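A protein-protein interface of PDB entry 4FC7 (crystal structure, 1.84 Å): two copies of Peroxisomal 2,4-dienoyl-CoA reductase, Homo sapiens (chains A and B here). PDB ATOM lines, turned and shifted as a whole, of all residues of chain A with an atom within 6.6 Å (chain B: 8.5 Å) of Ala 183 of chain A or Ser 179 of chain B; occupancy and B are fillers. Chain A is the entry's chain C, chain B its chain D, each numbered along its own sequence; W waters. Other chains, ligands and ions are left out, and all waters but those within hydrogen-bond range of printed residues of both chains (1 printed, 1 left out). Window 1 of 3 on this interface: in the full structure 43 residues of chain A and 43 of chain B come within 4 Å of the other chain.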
ATOM      1  N   MET A 133      -8.472   5.190   0.647  1.00  0.00           N
ATOM      2  CA  MET A 133      -8.567   5.023  -0.839  1.00  0.00           C
ATOM      3  C   MET A 133      -7.527   4.005  -1.298  1.00  0.00           C
ATOM      4  O   MET A 133      -7.790   3.154  -2.212  1.00  0.00           O
ATOM      5  CB  MET A 133      -8.282   6.332  -1.584  1.00  0.00           C
ATOM      6  CG  MET A 133      -9.333   7.391  -1.380  1.00  0.00           C
ATOM      7  SD  MET A 133     -10.931   7.046  -2.172  1.00  0.00           S
ATOM      8  CE  MET A 133     -11.939   7.465  -0.772  1.00  0.00           C
ATOM      9  N   THR A 137      -9.422   0.826  -2.693  1.00  0.00           N
ATOM     10  CA  THR A 137      -9.625   1.067  -4.076  1.00  0.00           C
ATOM     11  C   THR A 137      -8.423   0.667  -4.917  1.00  0.00           C
ATOM     12  O   THR A 137      -8.526  -0.213  -5.683  1.00  0.00           O
ATOM     13  CB  THR A 137     -10.095   2.495  -4.365  1.00  0.00           C
ATOM     14  OG1 THR A 137     -11.218   2.799  -3.551  1.00  0.00           O
ATOM     15  CG2 THR A 137     -10.511   2.552  -5.756  1.00  0.00           C
ATOM     16  N   GLY A 178     -16.989   5.285   2.484  1.00  0.00           N
ATOM     17  CA  GLY A 178     -18.046   5.461   1.450  1.00  0.00           C
ATOM     18  C   GLY A 178     -17.518   5.841   0.044  1.00  0.00           C
ATOM     19  O   GLY A 178     -18.033   5.332  -0.994  1.00  0.00           O
ATOM     20  N   SER A 179     -16.567   6.777  -0.028  1.00  0.00           N
ATOM     21  CA  SER A 179     -16.002   7.101  -1.334  1.00  0.00           C
ATOM     22  C   SER A 179     -15.273   5.922  -1.863  1.00  0.00           C
ATOM     23  O   SER A 179     -15.346   5.704  -3.089  1.00  0.00           O
ATOM     24  CB  SER A 179     -15.043   8.288  -1.254  1.00  0.00           C
ATOM     25  OG  SER A 179     -15.771   9.415  -0.707  1.00  0.00           O
ATOM     26  N   ALA A 180     -14.496   5.246  -1.020  1.00  0.00           N
ATOM     27  CA  ALA A 180     -13.587   4.134  -1.489  1.00  0.00           C
ATOM     28  C   ALA A 180     -14.450   3.002  -2.030  1.00  0.00           C
ATOM     29  O   ALA A 180     -14.215   2.446  -3.135  1.00  0.00           O
ATOM     30  CB  ALA A 180     -12.729   3.645  -0.315  1.00  0.00           C
ATOM     31  N   LYS A 181     -15.489   2.652  -1.278  1.00  0.00           N
ATOM     32  CA  LYS A 181     -16.315   1.570  -1.697  1.00  0.00           C
ATOM     33  C   LYS A 181     -17.182   1.915  -2.930  1.00  0.00           C
ATOM     34  O   LYS A 181     -17.583   1.040  -3.708  1.00  0.00           O
ATOM     35  CB  LYS A 181     -17.169   1.072  -0.514  1.00  0.00           C
ATOM     36  CG  LYS A 181     -16.374   0.415   0.624  1.00  0.00           C
ATOM     37  CD  LYS A 181     -15.288  -0.625   0.301  1.00  0.00           C
ATOM     38  CE  LYS A 181     -15.050  -1.516   1.578  1.00  0.00           C
ATOM     39  NZ  LYS A 181     -14.447  -2.887   1.320  1.00  0.00           N
ATOM     40  N   ALA A 182     -17.599   3.168  -3.057  1.00  0.00           N
ATOM     41  CA  ALA A 182     -18.322   3.554  -4.292  1.00  0.00           C
ATOM     42  C   ALA A 182     -17.398   3.446  -5.562  1.00  0.00           C
ATOM     43  O   ALA A 182     -17.868   3.093  -6.641  1.00  0.00           O
ATOM     44  CB  ALA A 182     -18.917   4.945  -4.227  1.00  0.00           C
ATOM     45  N   ALA A 183     -16.116   3.794  -5.423  1.00  0.00           N
ATOM     46  CA  ALA A 183     -15.159   3.566  -6.497  1.00  0.00           C
ATOM     47  C   ALA A 183     -15.076   2.040  -6.868  1.00  0.00           C
ATOM     48  O   ALA A 183     -15.036   1.717  -8.063  1.00  0.00           O
ATOM     49  CB  ALA A 183     -13.808   4.075  -6.105  1.00  0.00           C
ATOM     50  N   VAL A 184     -15.058   1.156  -5.857  1.00  0.00           N
ATOM     51  CA  VAL A 184     -14.939  -0.282  -6.131  1.00  0.00           C
ATOM     52  C   VAL A 184     -16.181  -0.767  -6.864  1.00  0.00           C
ATOM     53  O   VAL A 184     -16.090  -1.568  -7.835  1.00  0.00           O
ATOM     54  CB  VAL A 184     -14.684  -1.035  -4.814  1.00  0.00           C
ATOM     55  CG1 VAL A 184     -14.711  -2.559  -5.084  1.00  0.00           C
ATOM     56  CG2 VAL A 184     -13.289  -0.630  -4.223  1.00  0.00           C
ATOM     57  N   ASP A 185     -17.358  -0.301  -6.467  1.00  0.00           N
ATOM     58  CA  ASP A 185     -18.585  -0.581  -7.180  1.00  0.00           C
ATOM     59  C   ASP A 185     -18.526  -0.198  -8.660  1.00  0.00           C
ATOM     60  O   ASP A 185     -18.994  -0.971  -9.509  1.00  0.00           O
ATOM     61  CB  ASP A 185     -19.847   0.003  -6.505  1.00  0.00           C
ATOM     62  CG  ASP A 185     -20.277  -0.782  -5.205  1.00  0.00           C
ATOM     63  OD1 ASP A 185     -19.946  -2.007  -5.049  1.00  0.00           O
ATOM     64  OD2 ASP A 185     -20.960  -0.189  -4.290  1.00  0.00           O
ATOM     65  N   ALA A 186     -18.011   0.990  -8.959  1.00  0.00           N
ATOM     66  CA  ALA A 186     -17.844   1.414 -10.308  1.00  0.00           C
ATOM     67  C   ALA A 186     -16.789   0.551 -10.980  1.00  0.00           C
ATOM     68  O   ALA A 186     -16.937   0.144 -12.126  1.00  0.00           O
ATOM     69  CB  ALA A 186     -17.436   2.889 -10.371  1.00  0.00           C
ATOM     70  N   MET A 187     -15.740   0.254 -10.242  1.00  0.00           N
ATOM     71  CA  MET A 187     -14.703  -0.616 -10.789  1.00  0.00           C
ATOM     72  C   MET A 187     -15.246  -1.987 -11.200  1.00  0.00           C
ATOM     73  O   MET A 187     -14.833  -2.529 -12.268  1.00  0.00           O
ATOM     74  CB  MET A 187     -13.580  -0.831  -9.754  1.00  0.00           C
ATOM     75  CG  MET A 187     -12.307  -1.482 -10.323  1.00  0.00           C
ATOM     76  SD  MET A 187     -11.110  -1.978  -9.023  1.00  0.00           S
ATOM     77  CE  MET A 187     -11.116  -0.489  -7.969  1.00  0.00           C
ATOM     78  N   THR A 188     -16.176  -2.530 -10.417  1.00  0.00           N
ATOM     79  CA  THR A 188     -16.822  -3.779 -10.733  1.00  0.00           C
ATOM     80  C   THR A 188     -17.447  -3.751 -12.122  1.00  0.00           C
ATOM     81  O   THR A 188     -17.317  -4.711 -12.909  1.00  0.00           O
ATOM     82  CB  THR A 188     -17.894  -4.063  -9.713  1.00  0.00           C
ATOM     83  OG1 THR A 188     -17.200  -4.344  -8.508  1.00  0.00           O
ATOM     84  CG2 THR A 188     -18.800  -5.354 -10.164  1.00  0.00           C
ATOM     85  N   HIS A 190     -16.825  -1.513 -14.714  1.00  0.00           N
ATOM     86  CA  HIS A 190     -15.739  -1.345 -15.660  1.00  0.00           C
ATOM     87  C   HIS A 190     -15.053  -2.661 -15.977  1.00  0.00           C
ATOM     88  O   HIS A 190     -14.918  -3.022 -17.085  1.00  0.00           O
ATOM     89  CB  HIS A 190     -14.703  -0.339 -15.121  1.00  0.00           C
ATOM     90  CG  HIS A 190     -15.130   1.100 -15.209  1.00  0.00           C
ATOM     91  ND1 HIS A 190     -15.068   1.796 -16.315  1.00  0.00           N
ATOM     92  CD2 HIS A 190     -15.584   1.974 -14.223  1.00  0.00           C
ATOM     93  CE1 HIS A 190     -15.479   3.053 -16.076  1.00  0.00           C
ATOM     94  NE2 HIS A 190     -15.776   3.156 -14.792  1.00  0.00           N
ATOM     95  N   LEU B 124      -3.360  -0.835 -17.817  1.00  0.00           N
ATOM     96  CA  LEU B 124      -3.153   0.316 -16.887  1.00  0.00           C
ATOM     97  C   LEU B 124      -2.211  -0.071 -15.782  1.00  0.00           C
ATOM     98  O   LEU B 124      -2.500  -1.033 -15.048  1.00  0.00           O
ATOM     99  CB  LEU B 124      -4.520   0.671 -16.272  1.00  0.00           C
ATOM    100  CG  LEU B 124      -4.591   1.970 -15.472  1.00  0.00           C
ATOM    101  CD1 LEU B 124      -4.439   3.090 -16.475  1.00  0.00           C
ATOM    102  CD2 LEU B 124      -6.041   2.019 -14.930  1.00  0.00           C
ATOM    103  N   PHE B 129      -3.330   4.011 -12.347  1.00  0.00           N
ATOM    104  CA  PHE B 129      -4.571   4.020 -11.574  1.00  0.00           C
ATOM    105  C   PHE B 129      -4.547   4.932 -10.352  1.00  0.00           C
ATOM    106  O   PHE B 129      -5.476   5.760 -10.078  1.00  0.00           O
ATOM    107  CB  PHE B 129      -4.978   2.571 -11.179  1.00  0.00           C
ATOM    108  CG  PHE B 129      -6.356   2.493 -10.625  1.00  0.00           C
ATOM    109  CD1 PHE B 129      -7.435   2.307 -11.449  1.00  0.00           C
ATOM    110  CD2 PHE B 129      -6.561   2.592  -9.280  1.00  0.00           C
ATOM    111  CE1 PHE B 129      -8.723   2.219 -10.909  1.00  0.00           C
ATOM    112  CE2 PHE B 129      -7.854   2.540  -8.724  1.00  0.00           C
ATOM    113  CZ  PHE B 129      -8.922   2.374  -9.557  1.00  0.00           C
ATOM    114  N   VAL B 132      -4.633   8.728 -10.976  1.00  0.00           N
ATOM    115  CA  VAL B 132      -5.926   9.294 -11.314  1.00  0.00           C
ATOM    116  C   VAL B 132      -6.817   9.381 -10.034  1.00  0.00           C
ATOM    117  O   VAL B 132      -7.553  10.397  -9.828  1.00  0.00           O
ATOM    118  CB  VAL B 132      -6.586   8.553 -12.511  1.00  0.00           C
ATOM    119  CG1 VAL B 132      -8.077   8.945 -12.708  1.00  0.00           C
ATOM    120  CG2 VAL B 132      -5.815   8.853 -13.782  1.00  0.00           C
ATOM    121  N   MET B 133      -6.676   8.386  -9.146  1.00  0.00           N
ATOM    122  CA  MET B 133      -7.445   8.389  -7.924  1.00  0.00           C
ATOM    123  C   MET B 133      -6.932   9.537  -7.039  1.00  0.00           C
ATOM    124  O   MET B 133      -7.728  10.195  -6.405  1.00  0.00           O
ATOM    125  CB  MET B 133      -7.397   7.026  -7.224  1.00  0.00           C
ATOM    126  CG  MET B 133      -7.966   5.905  -8.095  1.00  0.00           C
ATOM    127  SD  MET B 133      -9.770   5.939  -8.279  1.00  0.00           S
ATOM    128  CE  MET B 133     -10.279   6.153  -6.559  1.00  0.00           C
ATOM    129  N   ASP B 136      -8.165  13.075  -8.774  1.00  0.00           N
ATOM    130  CA  ASP B 136      -9.610  13.369  -8.835  1.00  0.00           C
ATOM    131  C   ASP B 136     -10.229  13.269  -7.445  1.00  0.00           C
ATOM    132  O   ASP B 136     -11.103  14.062  -7.076  1.00  0.00           O
ATOM    133  CB  ASP B 136     -10.395  12.390  -9.711  1.00  0.00           C
ATOM    134  CG  ASP B 136     -10.106  12.539 -11.244  1.00  0.00           C
ATOM    135  OD1 ASP B 136      -9.092  13.144 -11.641  1.00  0.00           O
ATOM    136  OD2 ASP B 136     -10.898  11.936 -12.027  1.00  0.00           O
ATOM    137  N   THR B 137      -9.851  12.261  -6.706  1.00  0.00           N
ATOM    138  CA  THR B 137     -10.521  11.917  -5.503  1.00  0.00           C
ATOM    139  C   THR B 137      -9.873  12.520  -4.251  1.00  0.00           C
ATOM    140  O   THR B 137     -10.431  13.360  -3.644  1.00  0.00           O
ATOM    141  CB  THR B 137     -10.767  10.411  -5.361  1.00  0.00           C
ATOM    142  OG1 THR B 137     -11.196   9.821  -6.605  1.00  0.00           O
ATOM    143  CG2 THR B 137     -11.797  10.173  -4.360  1.00  0.00           C
ATOM    144  N   ALA B 164     -18.612  12.941 -13.533  1.00  0.00           N
ATOM    145  CA  ALA B 164     -18.730  12.317 -14.848  1.00  0.00           C
ATOM    146  C   ALA B 164     -19.720  11.190 -14.767  1.00  0.00           C
ATOM    147  O   ALA B 164     -20.099  10.758 -13.656  1.00  0.00           O
ATOM    148  CB  ALA B 164     -17.344  11.801 -15.339  1.00  0.00           C
ATOM    149  N   THR B 165     -20.119  10.648 -15.919  1.00  0.00           N
ATOM    150  CA  THR B 165     -21.084   9.537 -15.888  1.00  0.00           C
ATOM    151  C   THR B 165     -20.381   8.198 -16.185  1.00  0.00           C
ATOM    152  O   THR B 165     -21.065   7.159 -16.246  1.00  0.00           O
ATOM    153  CB  THR B 165     -22.190   9.773 -16.948  1.00  0.00           C
ATOM    154  OG1 THR B 165     -21.547   9.817 -18.229  1.00  0.00           O
ATOM    155  CG2 THR B 165     -22.956  11.149 -16.729  1.00  0.00           C
ATOM    156  N   LEU B 166     -19.054   8.205 -16.374  1.00  0.00           N
ATOM    157  CA  LEU B 166     -18.278   6.999 -16.847  1.00  0.00           C
ATOM    158  C   LEU B 166     -18.574   5.731 -16.021  1.00  0.00           C
ATOM    159  O   LEU B 166     -18.683   4.593 -16.574  1.00  0.00           O
ATOM    160  CB  LEU B 166     -16.781   7.283 -16.752  1.00  0.00           C
ATOM    161  CG  LEU B 166     -16.411   8.515 -17.573  1.00  0.00           C
ATOM    162  CD1 LEU B 166     -14.996   8.892 -17.133  1.00  0.00           C
ATOM    163  CD2 LEU B 166     -16.466   8.148 -19.072  1.00  0.00           C
ATOM    164  N   GLY B 167     -18.708   5.928 -14.688  1.00  0.00           N
ATOM    165  CA  GLY B 167     -18.856   4.817 -13.746  1.00  0.00           C
ATOM    166  C   GLY B 167     -20.204   4.156 -13.789  1.00  0.00           C
ATOM    167  O   GLY B 167     -20.338   3.038 -13.275  1.00  0.00           O
ATOM    168  N   ASN B 168     -21.210   4.861 -14.347  1.00  0.00           N
ATOM    169  CA  ASN B 168     -22.574   4.343 -14.434  1.00  0.00           C
ATOM    170  C   ASN B 168     -22.651   3.001 -15.177  1.00  0.00           C
ATOM    171  O   ASN B 168     -23.247   2.047 -14.623  1.00  0.00           O
ATOM    172  CB  ASN B 168     -23.561   5.341 -15.117  1.00  0.00           C
ATOM    173  CG  ASN B 168     -23.860   6.603 -14.274  1.00  0.00           C
ATOM    174  OD1 ASN B 168     -23.171   6.895 -13.268  1.00  0.00           O
ATOM    175  ND2 ASN B 168     -24.876   7.387 -14.717  1.00  0.00           N
ATOM    176  N   GLY B 170     -19.753   1.558 -16.539  1.00  0.00           N
ATOM    177  CA  GLY B 170     -18.407   1.049 -16.539  1.00  0.00           C
ATOM    178  C   GLY B 170     -17.815   1.197 -17.963  1.00  0.00           C
ATOM    179  O   GLY B 170     -17.406   0.195 -18.583  1.00  0.00           O
ATOM    180  N   GLN B 171     -17.777   2.438 -18.489  1.00  0.00           N
ATOM    181  CA  GLN B 171     -17.252   2.744 -19.821  1.00  0.00           C
ATOM    182  C   GLN B 171     -15.871   2.128 -20.096  1.00  0.00           C
ATOM    183  O   GLN B 171     -14.947   2.330 -19.322  1.00  0.00           O
ATOM    184  CB  GLN B 171     -17.187   4.285 -19.990  1.00  0.00           C
ATOM    185  CG  GLN B 171     -16.890   4.729 -21.435  1.00  0.00           C
ATOM    186  CD  GLN B 171     -18.004   4.291 -22.429  1.00  0.00           C
ATOM    187  OE1 GLN B 171     -19.162   4.238 -22.066  1.00  0.00           O
ATOM    188  NE2 GLN B 171     -17.638   3.983 -23.654  1.00  0.00           N
ATOM    189  N   GLN B 174     -11.696   3.241 -19.286  1.00  0.00           N
ATOM    190  CA  GLN B 174     -11.830   4.367 -18.376  1.00  0.00           C
ATOM    191  C   GLN B 174     -11.978   3.866 -16.963  1.00  0.00           C
ATOM    192  O   GLN B 174     -12.502   4.627 -16.087  1.00  0.00           O
ATOM    193  CB  GLN B 174     -13.086   5.178 -18.806  1.00  0.00           C
ATOM    194  CG  GLN B 174     -12.865   5.891 -20.117  1.00  0.00           C
ATOM    195  CD  GLN B 174     -12.086   7.145 -19.870  1.00  0.00           C
ATOM    196  OE1 GLN B 174     -10.838   7.110 -19.723  1.00  0.00           O
ATOM    197  NE2 GLN B 174     -12.799   8.261 -19.801  1.00  0.00           N
ATOM    198  N   VAL B 175     -11.423   2.692 -16.657  1.00  0.00           N
ATOM    199  CA  VAL B 175     -11.628   2.152 -15.209  1.00  0.00           C
ATOM    200  C   VAL B 175     -11.159   3.168 -14.126  1.00  0.00           C
ATOM    201  O   VAL B 175     -11.848   3.402 -13.080  1.00  0.00           O
ATOM    202  CB  VAL B 175     -11.043   0.745 -15.013  1.00  0.00           C
ATOM    203  CG1 VAL B 175      -9.522   0.775 -15.120  1.00  0.00           C
ATOM    204  CG2 VAL B 175     -11.568   0.110 -13.703  1.00  0.00           C
ATOM    205  N   HIS B 176      -9.995   3.772 -14.336  1.00  0.00           N
ATOM    206  CA  HIS B 176      -9.426   4.826 -13.447  1.00  0.00           C
ATOM    207  C   HIS B 176     -10.363   6.000 -13.245  1.00  0.00           C
ATOM    208  O   HIS B 176     -10.712   6.362 -12.096  1.00  0.00           O
ATOM    209  CB  HIS B 176      -8.023   5.295 -13.976  1.00  0.00           C
ATOM    210  CG  HIS B 176      -8.013   5.537 -15.479  1.00  0.00           C
ATOM    211  ND1 HIS B 176      -8.196   4.539 -16.370  1.00  0.00           N
ATOM    212  CD2 HIS B 176      -7.864   6.711 -16.228  1.00  0.00           C
ATOM    213  CE1 HIS B 176      -8.196   5.048 -17.619  1.00  0.00           C
ATOM    214  NE2 HIS B 176      -7.987   6.382 -17.521  1.00  0.00           N
ATOM    215  N   ALA B 177     -10.799   6.629 -14.352  1.00  0.00           N
ATOM    216  CA  ALA B 177     -11.604   7.861 -14.275  1.00  0.00           C
ATOM    217  C   ALA B 177     -13.021   7.547 -13.747  1.00  0.00           C
ATOM    218  O   ALA B 177     -13.583   8.283 -12.906  1.00  0.00           O
ATOM    219  CB  ALA B 177     -11.702   8.466 -15.682  1.00  0.00           C
ATOM    220  N   GLY B 178     -13.569   6.420 -14.166  1.00  0.00           N
ATOM    221  CA  GLY B 178     -14.887   5.975 -13.692  1.00  0.00           C
ATOM    222  C   GLY B 178     -14.957   5.725 -12.160  1.00  0.00           C
ATOM    223  O   GLY B 178     -15.941   6.161 -11.476  1.00  0.00           O
ATOM    224  N   SER B 179     -13.956   5.030 -11.669  1.00  0.00           N
ATOM    225  CA  SER B 179     -13.840   4.753 -10.285  1.00  0.00           C
ATOM    226  C   SER B 179     -13.704   6.098  -9.502  1.00  0.00           C
ATOM    227  O   SER B 179     -14.376   6.325  -8.559  1.00  0.00           O
ATOM    228  CB  SER B 179     -12.710   3.744 -10.029  1.00  0.00           C
ATOM    229  OG  SER B 179     -12.947   2.506 -10.681  1.00  0.00           O
ATOM    230  N   ALA B 180     -12.804   6.938  -9.963  1.00  0.00           N
ATOM    231  CA  ALA B 180     -12.478   8.194  -9.258  1.00  0.00           C
ATOM    232  C   ALA B 180     -13.678   9.117  -9.193  1.00  0.00           C
ATOM    233  O   ALA B 180     -13.943   9.739  -8.140  1.00  0.00           O
ATOM    234  CB  ALA B 180     -11.300   8.900  -9.938  1.00  0.00           C
ATOM    235  N   LYS B 181     -14.379   9.264 -10.307  1.00  0.00           N
ATOM    236  CA  LYS B 181     -15.531  10.117 -10.298  1.00  0.00           C
ATOM    237  C   LYS B 181     -16.719   9.545  -9.483  1.00  0.00           C
ATOM    238  O   LYS B 181     -17.448  10.321  -8.901  1.00  0.00           O
ATOM    239  CB  LYS B 181     -15.902  10.491 -11.727  1.00  0.00           C
ATOM    240  CG  LYS B 181     -14.750  11.273 -12.505  1.00  0.00           C
ATOM    241  CD  LYS B 181     -14.394  12.644 -11.835  1.00  0.00           C
ATOM    242  CE  LYS B 181     -13.818  13.578 -12.900  1.00  0.00           C
ATOM    243  NZ  LYS B 181     -13.547  15.027 -12.559  1.00  0.00           N
ATOM    244  N   ALA B 182     -16.952   8.216  -9.486  1.00  0.00           N
ATOM    245  CA  ALA B 182     -17.947   7.608  -8.637  1.00  0.00           C
ATOM    246  C   ALA B 182     -17.629   7.877  -7.093  1.00  0.00           C
ATOM    247  O   ALA B 182     -18.555   8.098  -6.306  1.00  0.00           O
ATOM    248  CB  ALA B 182     -18.019   6.127  -8.877  1.00  0.00           C
ATOM    249  N   ALA B 183     -16.339   7.836  -6.726  1.00  0.00           N
ATOM    250  CA  ALA B 183     -15.888   8.182  -5.406  1.00  0.00           C
ATOM    251  C   ALA B 183     -16.231   9.661  -5.159  1.00  0.00           C
ATOM    252  O   ALA B 183     -16.712   9.984  -4.051  1.00  0.00           O
ATOM    253  CB  ALA B 183     -14.370   7.958  -5.256  1.00  0.00           C
ATOM    254  N   VAL B 184     -16.040  10.531  -6.148  1.00  0.00           N
ATOM    255  CA  VAL B 184     -16.324  11.948  -5.807  1.00  0.00           C
ATOM    256  C   VAL B 184     -17.838  12.167  -5.659  1.00  0.00           C
ATOM    257  O   VAL B 184     -18.260  12.992  -4.851  1.00  0.00           O
ATOM    258  CB  VAL B 184     -15.743  12.910  -6.871  1.00  0.00           C
ATOM    259  CG1 VAL B 184     -16.247  14.331  -6.667  1.00  0.00           C
ATOM    260  CG2 VAL B 184     -14.219  12.921  -6.859  1.00  0.00           C
ATOM    261  N   ASP B 185     -18.675  11.504  -6.476  1.00  0.00           N
ATOM    262  CA  ASP B 185     -20.166  11.601  -6.274  1.00  0.00           C
ATOM    263  C   ASP B 185     -20.619  11.116  -4.912  1.00  0.00           C
ATOM    264  O   ASP B 185     -21.522  11.751  -4.287  1.00  0.00           O
ATOM    265  CB  ASP B 185     -20.963  10.803  -7.332  1.00  0.00           C
ATOM    266  CG  ASP B 185     -21.011  11.519  -8.692  1.00  0.00           C
ATOM    267  OD1 ASP B 185     -20.768  12.779  -8.740  1.00  0.00           O
ATOM    268  OD2 ASP B 185     -21.266  10.812  -9.763  1.00  0.00           O
ATOM    269  N   ALA B 186     -20.030  10.002  -4.427  1.00  0.00           N
ATOM    270  CA  ALA B 186     -20.281   9.552  -3.031  1.00  0.00           C
ATOM    271  C   ALA B 186     -19.781  10.655  -1.997  1.00  0.00           C
ATOM    272  O   ALA B 186     -20.504  11.018  -1.051  1.00  0.00           O
ATOM    273  CB  ALA B 186     -19.535   8.254  -2.733  1.00  0.00           C
ATOM    274  N   MET B 187     -18.554  11.183  -2.200  1.00  0.00           N
ATOM    275  CA  MET B 187     -18.071  12.246  -1.313  1.00  0.00           C
ATOM    276  C   MET B 187     -19.053  13.435  -1.261  1.00  0.00           C
ATOM    277  O   MET B 187     -19.198  14.034  -0.226  1.00  0.00           O
ATOM    278  CB  MET B 187     -16.690  12.711  -1.788  1.00  0.00           C
ATOM    279  CG  MET B 187     -16.050  13.671  -0.828  1.00  0.00           C
ATOM    280  SD  MET B 187     -14.552  14.333  -1.596  1.00  0.00           S
ATOM    281  CE  MET B 187     -13.725  12.898  -2.318  1.00  0.00           C
HETATM  282  O   HOH W   1     -12.983   0.294 -18.285  1.00  0.00           O
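A ring nitrogen (ND1) of His 190 of chain A sits at hydrogen-bond distance from the backbone carbonyl oxygen (O) of Gln 171 of chain B. OG of Ser 179 of chain B sits at hydrogen-bond distance from O of Ala 183 of chain A, 3.4 Å away.
O of Leu 166 of chain B sits at hydrogen-bond distance from N of Gln 171 of chain B, at 3.0 Å. OG of Ser 179 of chain B is in hydrogen-bond range of O of Val 175 of chain B, at 2.8 Å. The side-chain hydroxyl (OG1) of Thr 137 of chain B sits close to the backbone carbonyl oxygen (O) of Met 133 of chain B. N of Ala 180 of chain B sits at hydrogen-bond distance from SD of Met 133 of chain B (3.6 Å). The side-chain hydroxyl of Thr 137 of chain B is in hydrogen-bond range of the backbone carbonyl oxygen of Ala 180 of chain B (3.1 Å). OG1 of Thr 137 of chain A lies within hydrogen-bond range of O of Ala 180 of chain A (3.0 Å).
Met 133 of chain A touches Thr 137 of chain B. CG2 of Thr 137 of chain A touches CE of Met 133 of chain B, at 3.7 Å. Met 187 of chain B touches Ser 179 of chain A. O of Gly 178 of chain B touches CB of Ala 186 of chain A (3.8 Å). CB of Ala 182 of chain B touches CB of Ala 186 of chain A, 3.6 Å away. Met 187 of chain A touches Phe 129 of chain B (CE to CZ, 3.9 Å). CG of Met 187 of chain A touches CG2 of Val 175 of chain B, at 3.8 Å. Met 187 of chain A touches Ser 179 of chain B (CB to OG, 3.5 Å). C of Gly 170 of chain B touches ND1 of His 190 of chain A, at 3.3 Å. Val 175 of chain B touches His 190 of chain A.
Ala 180 of chain A touches none of the printed residues of chain B. Of the printed residues of chain B, Ala 183 of chain A touches Ser 179. Of the printed residues of chain A, Gly 167 of chain B touches His 190. Of the printed residues of chain A, Gln 171 of chain B touches His 190 (3.1 Å). Of the printed residues of chain A, Gln 174 of chain B touches His 190. Ser 179 of chain B touches just these residues of chain A: Ala 183 and Met 187. Val 184 of chain B touches none of the printed residues of chain A. Of the printed residues of chain A, Met 187 of chain B touches Ser 179. The nearest printed residue of chain A that does not touch Ser 179 of chain B is Ala 186 of chain A (4.1 Å). The nearest printed residue of chain A that does not touch Gly 170 of chain B is Ala 186 of chain A (4.7 Å).
Of the 14 printed residues of chain A, 9 touch a printed residue of chain B. Printed residues of chain A that touch a printed residue of chain B: Met 133, Thr 137, Gly 178, Ser 179, Ala 182, Ala 183, Ala 186, Met 187 and His 190. Along chain A the printed residues that touch a printed residue of chain B span positions 133 to 190. Of the 27 printed residues of chain B, 15 touch a printed residue of chain A. Hydrophobic or aromatic side chains of chain B that line the printed part of chain A: Phe 129, Met 133, Val 175, Ala 182, Ala 183, Ala 186 and Met 187.
Gly 178 of chain A touches Ala 186 of chain B, and with the chains exchanged Ala 186 of chain A touches Gly 178 of chain B. Ser 179 of chain A touches Met 187 of chain B, and with the chains exchanged Met 187 of chain A touches Ser 179 of chain B. Ala 182 of chain B touches its own counterpart, Ala 182 of chain A. Ala 182 of chain A touches Ala 186 of chain B, and with the chains exchanged Ala 186 of chain A touches Ala 182 of chain B. Of the 22 pairs that touch across the chains among the printed residues, 11 have their exchanged pair printed and touching as well.
Water W1 lies within hydrogen-bond range of the backbone carbonyl oxygen of Gln 171 of chain B (3.0 Å), a ring nitrogen (ND1) of His 190 of chain A (3.2 Å), the backbone NH of Val 175 of chain B (3.3 Å) and the backbone NH of Gln 174 of chain B (3.4 Å).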
